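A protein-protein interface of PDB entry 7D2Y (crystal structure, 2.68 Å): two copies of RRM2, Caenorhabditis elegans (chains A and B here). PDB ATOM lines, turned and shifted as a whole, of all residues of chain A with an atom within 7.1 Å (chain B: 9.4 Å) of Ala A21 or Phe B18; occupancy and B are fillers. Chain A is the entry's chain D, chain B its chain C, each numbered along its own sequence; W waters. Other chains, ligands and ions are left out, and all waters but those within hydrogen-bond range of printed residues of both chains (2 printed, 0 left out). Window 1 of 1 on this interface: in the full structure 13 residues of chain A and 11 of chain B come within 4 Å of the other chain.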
ATOM      1  N   LEU A  15      22.303  16.003  10.721  1.00  0.00           N
ATOM      2  CA  LEU A  15      22.088  16.495   9.363  1.00  0.00           C
ATOM      3  C   LEU A  15      23.122  15.923   8.420  1.00  0.00           C
ATOM      4  O   LEU A  15      24.325  16.043   8.673  1.00  0.00           O
ATOM      5  CB  LEU A  15      22.168  18.020   9.318  1.00  0.00           C
ATOM      6  CG  LEU A  15      21.118  18.746  10.135  1.00  0.00           C
ATOM      7  CD1 LEU A  15      21.113  20.184   9.741  1.00  0.00           C
ATOM      8  CD2 LEU A  15      19.758  18.127   9.923  1.00  0.00           C
ATOM      9  N   ASN A  16      22.660  15.318   7.317  1.00  0.00           N
ATOM     10  CA  ASN A  16      23.568  15.114   6.192  1.00  0.00           C
ATOM     11  C   ASN A  16      23.727  16.427   5.421  1.00  0.00           C
ATOM     12  O   ASN A  16      23.171  17.466   5.778  1.00  0.00           O
ATOM     13  CB  ASN A  16      23.112  13.948   5.310  1.00  0.00           C
ATOM     14  CG  ASN A  16      21.701  14.110   4.751  1.00  0.00           C
ATOM     15  OD1 ASN A  16      21.148  15.215   4.683  1.00  0.00           O
ATOM     16  ND2 ASN A  16      21.108  12.978   4.331  1.00  0.00           N
ATOM     17  N   THR A  17      24.536  16.404   4.371  1.00  0.00           N
ATOM     18  CA  THR A  17      24.799  17.653   3.674  1.00  0.00           C
ATOM     19  C   THR A  17      23.554  18.182   2.985  1.00  0.00           C
ATOM     20  O   THR A  17      23.413  19.392   2.845  1.00  0.00           O
ATOM     21  CB  THR A  17      25.916  17.478   2.669  1.00  0.00           C
ATOM     22  OG1 THR A  17      25.520  16.517   1.696  1.00  0.00           O
ATOM     23  CG2 THR A  17      27.159  16.982   3.358  1.00  0.00           C
ATOM     24  N   PHE A  18      22.625  17.314   2.579  1.00  0.00           N
ATOM     25  CA  PHE A  18      21.344  17.818   2.087  1.00  0.00           C
ATOM     26  C   PHE A  18      20.617  18.586   3.170  1.00  0.00           C
ATOM     27  O   PHE A  18      20.035  19.641   2.905  1.00  0.00           O
ATOM     28  CB  PHE A  18      20.468  16.675   1.588  1.00  0.00           C
ATOM     29  CG  PHE A  18      20.963  16.049   0.339  1.00  0.00           C
ATOM     30  CD1 PHE A  18      21.448  16.818  -0.682  1.00  0.00           C
ATOM     31  CD2 PHE A  18      20.965  14.687   0.188  1.00  0.00           C
ATOM     32  CE1 PHE A  18      21.895  16.234  -1.811  1.00  0.00           C
ATOM     33  CE2 PHE A  18      21.417  14.109  -0.971  1.00  0.00           C
ATOM     34  CZ  PHE A  18      21.876  14.885  -1.954  1.00  0.00           C
ATOM     35  N   GLY A  19      20.643  18.068   4.402  1.00  0.00           N
ATOM     36  CA  GLY A  19      20.034  18.771   5.517  1.00  0.00           C
ATOM     37  C   GLY A  19      20.712  20.093   5.815  1.00  0.00           C
ATOM     38  O   GLY A  19      20.064  21.057   6.230  1.00  0.00           O
ATOM     39  N   ILE A  20      22.026  20.169   5.606  1.00  0.00           N
ATOM     40  CA  ILE A  20      22.699  21.454   5.806  1.00  0.00           C
ATOM     41  C   ILE A  20      22.281  22.449   4.724  1.00  0.00           C
ATOM     42  O   ILE A  20      21.991  23.623   5.009  1.00  0.00           O
ATOM     43  CB  ILE A  20      24.228  21.269   5.857  1.00  0.00           C
ATOM     44  CG1 ILE A  20      24.621  20.509   7.123  1.00  0.00           C
ATOM     45  CG2 ILE A  20      24.948  22.609   5.770  1.00  0.00           C
ATOM     46  CD1 ILE A  20      25.958  19.834   7.042  1.00  0.00           C
ATOM     47  N   ALA A  21      22.220  21.992   3.468  1.00  0.00           N
ATOM     48  CA  ALA A  21      21.701  22.826   2.392  1.00  0.00           C
ATOM     49  C   ALA A  21      20.267  23.265   2.661  1.00  0.00           C
ATOM     50  O   ALA A  21      19.902  24.402   2.366  1.00  0.00           O
ATOM     51  CB  ALA A  21      21.803  22.084   1.068  1.00  0.00           C
ATOM     52  N   GLN A  22      19.441  22.388   3.234  1.00  0.00           N
ATOM     53  CA  GLN A  22      18.077  22.784   3.561  1.00  0.00           C
ATOM     54  C   GLN A  22      18.040  23.963   4.532  1.00  0.00           C
ATOM     55  O   GLN A  22      17.109  24.777   4.484  1.00  0.00           O
ATOM     56  CB  GLN A  22      17.317  21.601   4.136  1.00  0.00           C
ATOM     57  CG  GLN A  22      16.873  20.650   3.098  1.00  0.00           C
ATOM     58  CD  GLN A  22      16.330  19.337   3.638  1.00  0.00           C
ATOM     59  OE1 GLN A  22      16.653  18.907   4.758  1.00  0.00           O
ATOM     60  NE2 GLN A  22      15.491  18.687   2.833  1.00  0.00           N
ATOM     61  N   LEU A  23      19.024  24.065   5.431  1.00  0.00           N
ATOM     62  CA  LEU A  23      19.079  25.198   6.350  1.00  0.00           C
ATOM     63  C   LEU A  23      19.187  26.525   5.613  1.00  0.00           C
ATOM     64  O   LEU A  23      18.712  27.550   6.104  1.00  0.00           O
ATOM     65  CB  LEU A  23      20.273  25.052   7.289  1.00  0.00           C
ATOM     66  CG  LEU A  23      20.255  23.993   8.394  1.00  0.00           C
ATOM     67  CD1 LEU A  23      21.595  24.017   9.085  1.00  0.00           C
ATOM     68  CD2 LEU A  23      19.131  24.196   9.410  1.00  0.00           C
ATOM     69  N   LEU A  24      19.821  26.536   4.449  1.00  0.00           N
ATOM     70  CA  LEU A  24      20.158  27.773   3.773  1.00  0.00           C
ATOM     71  C   LEU A  24      19.158  28.152   2.690  1.00  0.00           C
ATOM     72  O   LEU A  24      19.406  29.104   1.958  1.00  0.00           O
ATOM     73  CB  LEU A  24      21.559  27.672   3.194  1.00  0.00           C
ATOM     74  CG  LEU A  24      22.655  27.454   4.228  1.00  0.00           C
ATOM     75  CD1 LEU A  24      23.943  27.032   3.548  1.00  0.00           C
ATOM     76  CD2 LEU A  24      22.868  28.728   5.022  1.00  0.00           C
ATOM     77  N   THR A  25      18.033  27.448   2.578  1.00  0.00           N
ATOM     78  CA  THR A  25      16.926  27.835   1.702  1.00  0.00           C
ATOM     79  C   THR A  25      16.682  29.328   1.852  1.00  0.00           C
ATOM     80  O   THR A  25      16.540  29.806   2.976  1.00  0.00           O
ATOM     81  CB  THR A  25      15.640  27.066   2.031  1.00  0.00           C
ATOM     82  OG1 THR A  25      15.956  25.700   2.288  1.00  0.00           O
ATOM     83  CG2 THR A  25      14.700  27.095   0.881  1.00  0.00           C
ATOM     84  N   PRO A  26      16.579  30.102   0.764  1.00  0.00           N
ATOM     85  CA  PRO A  26      16.524  29.710  -0.642  1.00  0.00           C
ATOM     86  C   PRO A  26      17.824  29.936  -1.399  1.00  0.00           C
ATOM     87  O   PRO A  26      17.856  29.811  -2.620  1.00  0.00           O
ATOM     88  CB  PRO A  26      15.436  30.618  -1.169  1.00  0.00           C
ATOM     89  CG  PRO A  26      15.688  31.899  -0.448  1.00  0.00           C
ATOM     90  CD  PRO A  26      16.250  31.529   0.918  1.00  0.00           C
ATOM     91  N   TYR A  27      18.885  30.271  -0.677  1.00  0.00           N
ATOM     92  CA  TYR A  27      20.158  30.548  -1.318  1.00  0.00           C
ATOM     93  C   TYR A  27      20.706  29.306  -2.003  1.00  0.00           C
ATOM     94  O   TYR A  27      20.602  28.186  -1.488  1.00  0.00           O
ATOM     95  CB  TYR A  27      21.138  31.084  -0.293  1.00  0.00           C
ATOM     96  CG  TYR A  27      20.580  32.334   0.332  1.00  0.00           C
ATOM     97  CD1 TYR A  27      20.517  33.530  -0.402  1.00  0.00           C
ATOM     98  CD2 TYR A  27      20.075  32.329   1.638  1.00  0.00           C
ATOM     99  CE1 TYR A  27      19.997  34.678   0.149  1.00  0.00           C
ATOM    100  CE2 TYR A  27      19.546  33.487   2.193  1.00  0.00           C
ATOM    101  CZ  TYR A  27      19.510  34.658   1.439  1.00  0.00           C
ATOM    102  OH  TYR A  27      18.996  35.824   1.962  1.00  0.00           O
ATOM    103  N   ARG A  28      21.299  29.519  -3.173  1.00  0.00           N
ATOM    104  CA  ARG A  28      21.836  28.423  -3.956  1.00  0.00           C
ATOM    105  C   ARG A  28      23.141  27.919  -3.344  1.00  0.00           C
ATOM    106  O   ARG A  28      24.085  28.692  -3.172  1.00  0.00           O
ATOM    107  CB  ARG A  28      22.055  28.879  -5.398  1.00  0.00           C
ATOM    108  CG  ARG A  28      22.809  27.871  -6.213  1.00  0.00           C
ATOM    109  CD  ARG A  28      22.615  28.062  -7.674  1.00  0.00           C
ATOM    110  NE  ARG A  28      23.558  27.253  -8.448  1.00  0.00           N
ATOM    111  CZ  ARG A  28      23.210  26.301  -9.307  1.00  0.00           C
ATOM    112  NH1 ARG A  28      21.936  26.031  -9.524  1.00  0.00           N
ATOM    113  NH2 ARG A  28      24.142  25.631  -9.969  1.00  0.00           N
ATOM    114  N   VAL A  29      23.203  26.618  -3.060  1.00  0.00           N
ATOM    115  CA  VAL A  29      24.380  25.948  -2.520  1.00  0.00           C
ATOM    116  C   VAL A  29      25.078  25.178  -3.631  1.00  0.00           C
ATOM    117  O   VAL A  29      24.452  24.363  -4.326  1.00  0.00           O
ATOM    118  CB  VAL A  29      23.992  24.975  -1.392  1.00  0.00           C
ATOM    119  CG1 VAL A  29      25.202  24.179  -0.964  1.00  0.00           C
ATOM    120  CG2 VAL A  29      23.355  25.702  -0.226  1.00  0.00           C
ATOM    121  N   ASN A  30      26.387  25.372  -3.764  1.00  0.00           N
ATOM    122  CA  ASN A  30      27.154  24.624  -4.750  1.00  0.00           C
ATOM    123  C   ASN A  30      27.995  23.499  -4.167  1.00  0.00           C
ATOM    124  O   ASN A  30      28.143  22.459  -4.804  1.00  0.00           O
ATOM    125  CB  ASN A  30      28.048  25.572  -5.527  1.00  0.00           C
ATOM    126  CG  ASN A  30      27.248  26.511  -6.379  1.00  0.00           C
ATOM    127  OD1 ASN A  30      26.182  26.142  -6.834  1.00  0.00           O
ATOM    128  ND2 ASN A  30      27.737  27.730  -6.589  1.00  0.00           N
ATOM    129  N   GLY A  31      28.558  23.671  -2.986  1.00  0.00           N
ATOM    130  CA  GLY A  31      29.312  22.599  -2.365  1.00  0.00           C
ATOM    131  C   GLY A  31      29.262  22.730  -0.870  1.00  0.00           C
ATOM    132  O   GLY A  31      29.098  23.831  -0.330  1.00  0.00           O
ATOM    133  N   ILE A  32      29.391  21.598  -0.181  1.00  0.00           N
ATOM    134  CA  ILE A  32      29.444  21.564   1.272  1.00  0.00           C
ATOM    135  C   ILE A  32      30.587  20.648   1.678  1.00  0.00           C
ATOM    136  O   ILE A  32      30.685  19.522   1.180  1.00  0.00           O
ATOM    137  CB  ILE A  32      28.118  21.091   1.897  1.00  0.00           C
ATOM    138  CG1 ILE A  32      26.974  21.997   1.436  1.00  0.00           C
ATOM    139  CG2 ILE A  32      28.223  21.073   3.403  1.00  0.00           C
ATOM    140  CD1 ILE A  32      25.647  21.696   2.063  1.00  0.00           C
ATOM    141  N   VAL A  42      30.521  26.014   3.475  1.00  0.00           N
ATOM    142  CA  VAL A  42      29.538  25.995   2.398  1.00  0.00           C
ATOM    143  C   VAL A  42      29.932  27.003   1.324  1.00  0.00           C
ATOM    144  O   VAL A  42      30.204  28.171   1.627  1.00  0.00           O
ATOM    145  CB  VAL A  42      28.123  26.306   2.921  1.00  0.00           C
ATOM    146  CG1 VAL A  42      27.134  26.311   1.773  1.00  0.00           C
ATOM    147  CG2 VAL A  42      27.720  25.293   3.956  1.00  0.00           C
ATOM    148  N   ALA A  43      29.935  26.561   0.079  1.00  0.00           N
ATOM    149  CA  ALA A  43      30.106  27.434  -1.076  1.00  0.00           C
ATOM    150  C   ALA A  43      28.724  27.828  -1.609  1.00  0.00           C
ATOM    151  O   ALA A  43      27.981  26.982  -2.116  1.00  0.00           O
ATOM    152  CB  ALA A  43      30.930  26.729  -2.150  1.00  0.00           C
ATOM    153  N   MET B  14      16.804  25.502 -13.300  1.00  0.00           N
ATOM    154  CA  MET B  14      18.167  25.840 -12.897  1.00  0.00           C
ATOM    155  C   MET B  14      18.626  25.133 -11.606  1.00  0.00           C
ATOM    156  O   MET B  14      19.829  25.158 -11.307  1.00  0.00           O
ATOM    157  CB  MET B  14      18.275  27.356 -12.745  1.00  0.00           C
ATOM    158  CG  MET B  14      17.031  27.972 -12.073  1.00  0.00           C
ATOM    159  SD  MET B  14      17.256  29.460 -11.051  1.00  0.00           S
ATOM    160  CE  MET B  14      18.522  28.921  -9.882  1.00  0.00           C
ATOM    161  N   LEU B  15      17.721  24.501 -10.853  1.00  0.00           N
ATOM    162  CA  LEU B  15      18.099  23.849  -9.609  1.00  0.00           C
ATOM    163  C   LEU B  15      19.165  22.780  -9.831  1.00  0.00           C
ATOM    164  O   LEU B  15      19.154  22.060 -10.836  1.00  0.00           O
ATOM    165  CB  LEU B  15      16.877  23.222  -8.950  1.00  0.00           C
ATOM    166  CG  LEU B  15      15.706  24.117  -8.552  1.00  0.00           C
ATOM    167  CD1 LEU B  15      14.743  23.292  -7.728  1.00  0.00           C
ATOM    168  CD2 LEU B  15      16.140  25.340  -7.795  1.00  0.00           C
ATOM    169  N   ASN B  16      20.117  22.709  -8.896  1.00  0.00           N
ATOM    170  CA  ASN B  16      21.050  21.603  -8.790  1.00  0.00           C
ATOM    171  C   ASN B  16      20.525  20.644  -7.711  1.00  0.00           C
ATOM    172  O   ASN B  16      19.471  20.869  -7.109  1.00  0.00           O
ATOM    173  CB  ASN B  16      22.471  22.123  -8.531  1.00  0.00           C
ATOM    174  CG  ASN B  16      22.580  22.996  -7.277  1.00  0.00           C
ATOM    175  OD1 ASN B  16      21.709  22.976  -6.396  1.00  0.00           O
ATOM    176  ND2 ASN B  16      23.681  23.766  -7.183  1.00  0.00           N
ATOM    177  N   THR B  17      21.248  19.547  -7.463  1.00  0.00           N
ATOM    178  CA  THR B  17      20.711  18.578  -6.520  1.00  0.00           C
ATOM    179  C   THR B  17      20.504  19.192  -5.130  1.00  0.00           C
ATOM    180  O   THR B  17      19.501  18.897  -4.479  1.00  0.00           O
ATOM    181  CB  THR B  17      21.574  17.307  -6.467  1.00  0.00           C
ATOM    182  OG1 THR B  17      22.747  17.533  -5.687  1.00  0.00           O
ATOM    183  CG2 THR B  17      22.005  16.911  -7.834  1.00  0.00           C
ATOM    184  N   PHE B  18      21.388  20.085  -4.664  1.00  0.00           N
ATOM    185  CA  PHE B  18      21.091  20.751  -3.386  1.00  0.00           C
ATOM    186  C   PHE B  18      19.783  21.526  -3.463  1.00  0.00           C
ATOM    187  O   PHE B  18      18.980  21.490  -2.524  1.00  0.00           O
ATOM    188  CB  PHE B  18      22.201  21.712  -2.954  1.00  0.00           C
ATOM    189  CG  PHE B  18      23.442  21.033  -2.466  1.00  0.00           C
ATOM    190  CD1 PHE B  18      23.404  20.177  -1.395  1.00  0.00           C
ATOM    191  CD2 PHE B  18      24.656  21.259  -3.079  1.00  0.00           C
ATOM    192  CE1 PHE B  18      24.537  19.556  -0.970  1.00  0.00           C
ATOM    193  CE2 PHE B  18      25.786  20.642  -2.636  1.00  0.00           C
ATOM    194  CZ  PHE B  18      25.722  19.794  -1.594  1.00  0.00           C
ATOM    195  N   GLY B  19      19.548  22.232  -4.576  1.00  0.00           N
ATOM    196  CA  GLY B  19      18.326  23.018  -4.704  1.00  0.00           C
ATOM    197  C   GLY B  19      17.065  22.166  -4.737  1.00  0.00           C
ATOM    198  O   GLY B  19      16.016  22.575  -4.229  1.00  0.00           O
ATOM    199  N   ILE B  20      17.135  20.987  -5.369  1.00  0.00           N
ATOM    200  CA  ILE B  20      16.021  20.041  -5.292  1.00  0.00           C
ATOM    201  C   ILE B  20      15.801  19.621  -3.844  1.00  0.00           C
ATOM    202  O   ILE B  20      14.660  19.473  -3.386  1.00  0.00           O
ATOM    203  CB  ILE B  20      16.266  18.817  -6.211  1.00  0.00           C
ATOM    204  CG1 ILE B  20      16.247  19.208  -7.699  1.00  0.00           C
ATOM    205  CG2 ILE B  20      15.225  17.727  -5.967  1.00  0.00           C
ATOM    206  CD1 ILE B  20      17.117  18.354  -8.558  1.00  0.00           C
ATOM    207  N   ALA B  21      16.889  19.437  -3.092  1.00  0.00           N
ATOM    208  CA  ALA B  21      16.737  19.067  -1.682  1.00  0.00           C
ATOM    209  C   ALA B  21      16.076  20.189  -0.888  1.00  0.00           C
ATOM    210  O   ALA B  21      15.225  19.930  -0.031  1.00  0.00           O
ATOM    211  CB  ALA B  21      18.086  18.706  -1.057  1.00  0.00           C
ATOM    212  N   GLN B  22      16.444  21.442  -1.180  1.00  0.00           N
ATOM    213  CA  GLN B  22      15.801  22.576  -0.527  1.00  0.00           C
ATOM    214  C   GLN B  22      14.303  22.592  -0.795  1.00  0.00           C
ATOM    215  O   GLN B  22      13.517  22.923   0.100  1.00  0.00           O
ATOM    216  CB  GLN B  22      16.465  23.880  -0.970  1.00  0.00           C
ATOM    217  CG  GLN B  22      17.825  24.095  -0.325  1.00  0.00           C
ATOM    218  CD  GLN B  22      18.695  25.088  -1.040  1.00  0.00           C
ATOM    219  OE1 GLN B  22      18.765  25.105  -2.268  1.00  0.00           O
ATOM    220  NE2 GLN B  22      19.368  25.930  -0.281  1.00  0.00           N
ATOM    221  N   LEU B  23      13.880  22.216  -2.010  1.00  0.00           N
ATOM    222  CA  LEU B  23      12.449  22.137  -2.285  1.00  0.00           C
ATOM    223  C   LEU B  23      11.739  21.309  -1.239  1.00  0.00           C
ATOM    224  O   LEU B  23      10.605  21.614  -0.870  1.00  0.00           O
ATOM    225  CB  LEU B  23      12.158  21.500  -3.632  1.00  0.00           C
ATOM    226  CG  LEU B  23      12.305  22.203  -4.943  1.00  0.00           C
ATOM    227  CD1 LEU B  23      11.911  21.168  -5.973  1.00  0.00           C
ATOM    228  CD2 LEU B  23      11.441  23.430  -5.013  1.00  0.00           C
ATOM    229  N   LEU B  24      12.383  20.246  -0.767  1.00  0.00           N
ATOM    230  CA  LEU B  24      11.728  19.232   0.035  1.00  0.00           C
ATOM    231  C   LEU B  24      11.820  19.498   1.532  1.00  0.00           C
ATOM    232  O   LEU B  24      11.462  18.615   2.319  1.00  0.00           O
ATOM    233  CB  LEU B  24      12.312  17.854  -0.319  1.00  0.00           C
ATOM    234  CG  LEU B  24      11.990  17.448  -1.780  1.00  0.00           C
ATOM    235  CD1 LEU B  24      12.718  16.209  -2.251  1.00  0.00           C
ATOM    236  CD2 LEU B  24      10.493  17.277  -1.926  1.00  0.00           C
ATOM    237  N   THR B  25      12.270  20.679   1.946  1.00  0.00           N
ATOM    238  CA  THR B  25      12.386  20.982   3.367  1.00  0.00           C
ATOM    239  C   THR B  25      11.045  20.783   4.075  1.00  0.00           C
ATOM    240  O   THR B  25      10.016  21.262   3.580  1.00  0.00           O
ATOM    241  CB  THR B  25      12.856  22.418   3.550  1.00  0.00           C
ATOM    242  OG1 THR B  25      14.124  22.564   2.934  1.00  0.00           O
ATOM    243  CG2 THR B  25      13.037  22.730   4.960  1.00  0.00           C
ATOM    244  N   TYR B  27      11.965  17.447   5.026  1.00  0.00           N
ATOM    245  CA  TYR B  27      12.146  15.996   5.009  1.00  0.00           C
ATOM    246  C   TYR B  27      13.592  15.599   4.714  1.00  0.00           C
ATOM    247  O   TYR B  27      14.318  16.303   4.018  1.00  0.00           O
ATOM    248  CB  TYR B  27      11.211  15.372   3.971  1.00  0.00           C
ATOM    249  CG  TYR B  27       9.796  15.714   4.317  1.00  0.00           C
ATOM    250  CD1 TYR B  27       9.228  15.222   5.474  1.00  0.00           C
ATOM    251  CD2 TYR B  27       9.061  16.593   3.540  1.00  0.00           C
ATOM    252  CE1 TYR B  27       7.971  15.551   5.833  1.00  0.00           C
ATOM    253  CE2 TYR B  27       7.789  16.922   3.881  1.00  0.00           C
ATOM    254  CZ  TYR B  27       7.248  16.393   5.043  1.00  0.00           C
ATOM    255  OH  TYR B  27       5.979  16.718   5.438  1.00  0.00           O
ATOM    256  N   VAL B  29      16.504  13.991   2.964  1.00  0.00           N
ATOM    257  CA  VAL B  29      16.860  13.495   1.649  1.00  0.00           C
ATOM    258  C   VAL B  29      18.127  12.667   1.785  1.00  0.00           C
ATOM    259  O   VAL B  29      19.131  13.146   2.318  1.00  0.00           O
ATOM    260  CB  VAL B  29      17.063  14.659   0.670  1.00  0.00           C
ATOM    261  CG1 VAL B  29      17.516  14.133  -0.658  1.00  0.00           C
ATOM    262  CG2 VAL B  29      15.766  15.441   0.553  1.00  0.00           C
ATOM    263  N   GLY B  31      19.168  10.638  -1.130  1.00  0.00           N
ATOM    264  CA  GLY B  31      19.734  10.605  -2.461  1.00  0.00           C
ATOM    265  C   GLY B  31      18.813  11.272  -3.444  1.00  0.00           C
ATOM    266  O   GLY B  31      17.588  11.229  -3.303  1.00  0.00           O
ATOM    267  N   ILE B  32      19.404  11.917  -4.442  1.00  0.00           N
ATOM    268  CA  ILE B  32      18.683  12.471  -5.576  1.00  0.00           C
ATOM    269  C   ILE B  32      19.320  11.931  -6.842  1.00  0.00           C
ATOM    270  O   ILE B  32      20.540  12.012  -7.004  1.00  0.00           O
ATOM    271  CB  ILE B  32      18.722  14.005  -5.581  1.00  0.00           C
ATOM    272  CG1 ILE B  32      18.325  14.538  -4.202  1.00  0.00           C
ATOM    273  CG2 ILE B  32      17.831  14.522  -6.702  1.00  0.00           C
ATOM    274  CD1 ILE B  32      18.046  16.020  -4.180  1.00  0.00           C
ATOM    275  N   ILE B  34      19.425  12.506 -10.759  1.00  0.00           N
ATOM    276  CA  ILE B  34      19.058  13.392 -11.857  1.00  0.00           C
ATOM    277  C   ILE B  34      19.360  12.684 -13.173  1.00  0.00           C
ATOM    278  O   ILE B  34      20.384  11.994 -13.308  1.00  0.00           O
ATOM    279  CB  ILE B  34      19.793  14.742 -11.719  1.00  0.00           C
ATOM    280  CG1 ILE B  34      21.269  14.492 -11.464  1.00  0.00           C
ATOM    281  CG2 ILE B  34      19.228  15.541 -10.557  1.00  0.00           C
ATOM    282  CD1 ILE B  34      22.056  14.544 -12.734  1.00  0.00           C
ATOM    283  N   VAL B  42      13.841  11.006  -5.932  1.00  0.00           N
ATOM    284  CA  VAL B  42      14.438  11.352  -4.643  1.00  0.00           C
ATOM    285  C   VAL B  42      14.177  10.215  -3.663  1.00  0.00           C
ATOM    286  O   VAL B  42      13.047   9.728  -3.545  1.00  0.00           O
ATOM    287  CB  VAL B  42      13.874  12.680  -4.094  1.00  0.00           C
ATOM    288  CG1 VAL B  42      14.405  12.927  -2.686  1.00  0.00           C
ATOM    289  CG2 VAL B  42      14.234  13.856  -4.991  1.00  0.00           C
HETATM  290  O   HOH W   1      18.138  16.024   4.225  1.00  0.00           O
HETATM  291  O   HOH W   2      20.845  25.302  -4.057  1.00  0.00           O
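The guanidinium group (NH1) of Arg A28 sits at hydrogen-bond distance from the backbone carbonyl oxygen (O) of Met B14 (2.9 Å). The side-chain amide nitrogen (ND2) of Asn B16 lies close to the guanidinium group (NH2) of Arg A28 (3.4 Å). O of Tyr B27 sits at hydrogen-bond distance from NE2 of Gln A22. O of Val B29 lies within hydrogen-bond range of ND2 of Asn A16 (2.8 Å). The side-chain amide nitrogen (ND2) of Asn B16 sits at hydrogen-bond distance from the backbone carbonyl oxygen (O) of Val A29 (3.0 Å). The side-chain amide nitrogen (NE2) of Gln B22 sits at hydrogen-bond distance from the backbone carbonyl oxygen (O) of Ala A21 (3.1 Å). ND2 of Asn B16 is in hydrogen-bond range of OD1 of Asn A30, 3.5 Å away. NE2 of Gln B22 lies within hydrogen-bond range of O of Tyr A27 (2.8 Å). The backbone carbonyl oxygen of Ala B21 lies within hydrogen-bond range of the side-chain amide nitrogen of Gln A22 (3.1 Å).
OD1 of Asn B16 lies close to N of Phe B18, 3.4 Å away. The guanidinium group (NE) of Arg A28 lies within hydrogen-bond range of the side-chain amide oxygen (OD1) of Asn A30. The backbone NH (N) of Asn A30 lies within hydrogen-bond range of the backbone carbonyl oxygen (O) of Ala A43, 2.8 Å away. The side-chain amide oxygen (OD1) of Asn A16 sits close to the backbone NH (N) of Phe A18. The backbone carbonyl oxygen (O) of Gln B22 is in hydrogen-bond range of the side-chain hydroxyl (OG1) of Thr B25, at 2.9 Å. O of Gln A22 sits at hydrogen-bond distance from OG1 of Thr A25.
Thr A17 touches Phe B18 (O to CE1, 3.98 Å). CD2 of Phe A18 touches O of Val B29 (3.2 Å). Ala A21 touches Phe B18. Gln A22 touches Val B29 (NE2 to CG2, 3.98 Å). Gln B22 touches Leu A24 (NE2 to C, 3.7 Å). Thr A25 touches Thr B25 (OG1 to OG1, 3.7 Å). Val A29 touches Phe B18 (O to CD2, 3.4 Å). Val A29 touches Gln B22. Phe B18 touches Asn A30 (CE2 to O, 3.7 Å). Ile A32 touches Phe B18 (CD1 to CE1, 3.9 Å).
Of chain B, only Phe B18 and Gln B22 come within 4 Å of Ala A21. Of the printed residues of chain A, Phe B18 touches Thr A17 (3.98 Å), Phe A18 (3.95 Å), Ala A21 (3.5 Å), Val A29 (3.4 Å), Asn A30 (3.7 Å) and Ile A32 (3.9 Å). No residue of chain B comes within 4 Å of Gly A19. Gly A31 touches none of the printed residues of chain B. Of the printed residues of chain A, Gln B22 touches Ala A21 (3.1 Å), Leu A24 (3.7 Å), Thr A25 (3.5 Å), Tyr A27 (2.8 Å) and Val A29 (3.99 Å). Printed residues of chain B within 4 Å of Asn A30: Asn B16 (3.5 Å) and Phe B18 (3.7 Å). Of the printed residues of chain B, Asn A16 touches Val B29 (2.8 Å). Of the printed residues of chain B, Thr A17 touches Phe B18 (3.98 Å). Ile A20 touches none of the printed residues of chain B. The nearest printed residue of chain A that does not touch Phe B18 is Gly A31 (4.04 Å).
Of the 18 printed residues of chain B, 9 touch a printed residue of chain A. Printed residues of chain B that touch a printed residue of chain A: Met B14, Asn B16, Phe B18, Ala B21, Gln B22, Leu B24, Thr B25, Tyr B27 and Val B29. Hydrophobic or aromatic side chains of chain B within 4 Å of the printed part of chain A: Phe B18, Ala B21 and Val B29. Along chain B the printed residues that touch a printed residue of chain A span positions 14 to 29. Among the printed residues, 24 pairs touch across the chains.
Asn A16 touches Val B29, and with the chains exchanged Val A29 touches Asn B16. Phe A18 touches Val B29, and with the chains exchanged Val A29 touches Phe B18. Gln A22 touches Leu B24, and with the chains exchanged Leu A24 touches Gln B22. Gln A22 touches Tyr B27, and with the chains exchanged Tyr A27 touches Gln B22. Of the 24 pairs that touch across the chains among the printed residues, 18 have their exchanged pair printed and touching as well.
Water W2 lies within hydrogen-bond range of the side-chain amide oxygen (OE1) of Gln B22, the backbone NH (N) of Val A29, the backbone NH (N) of Gly B19 and the side-chain amide oxygen (OD1) of Asn B16. Water W1 lies within hydrogen-bond range of the backbone NH (N) of Val B29, the side-chain amide oxygen (OD1) of Asn A16, the backbone NH (N) of Gly A19 and the side-chain amide oxygen (OE1) of Gln A22.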
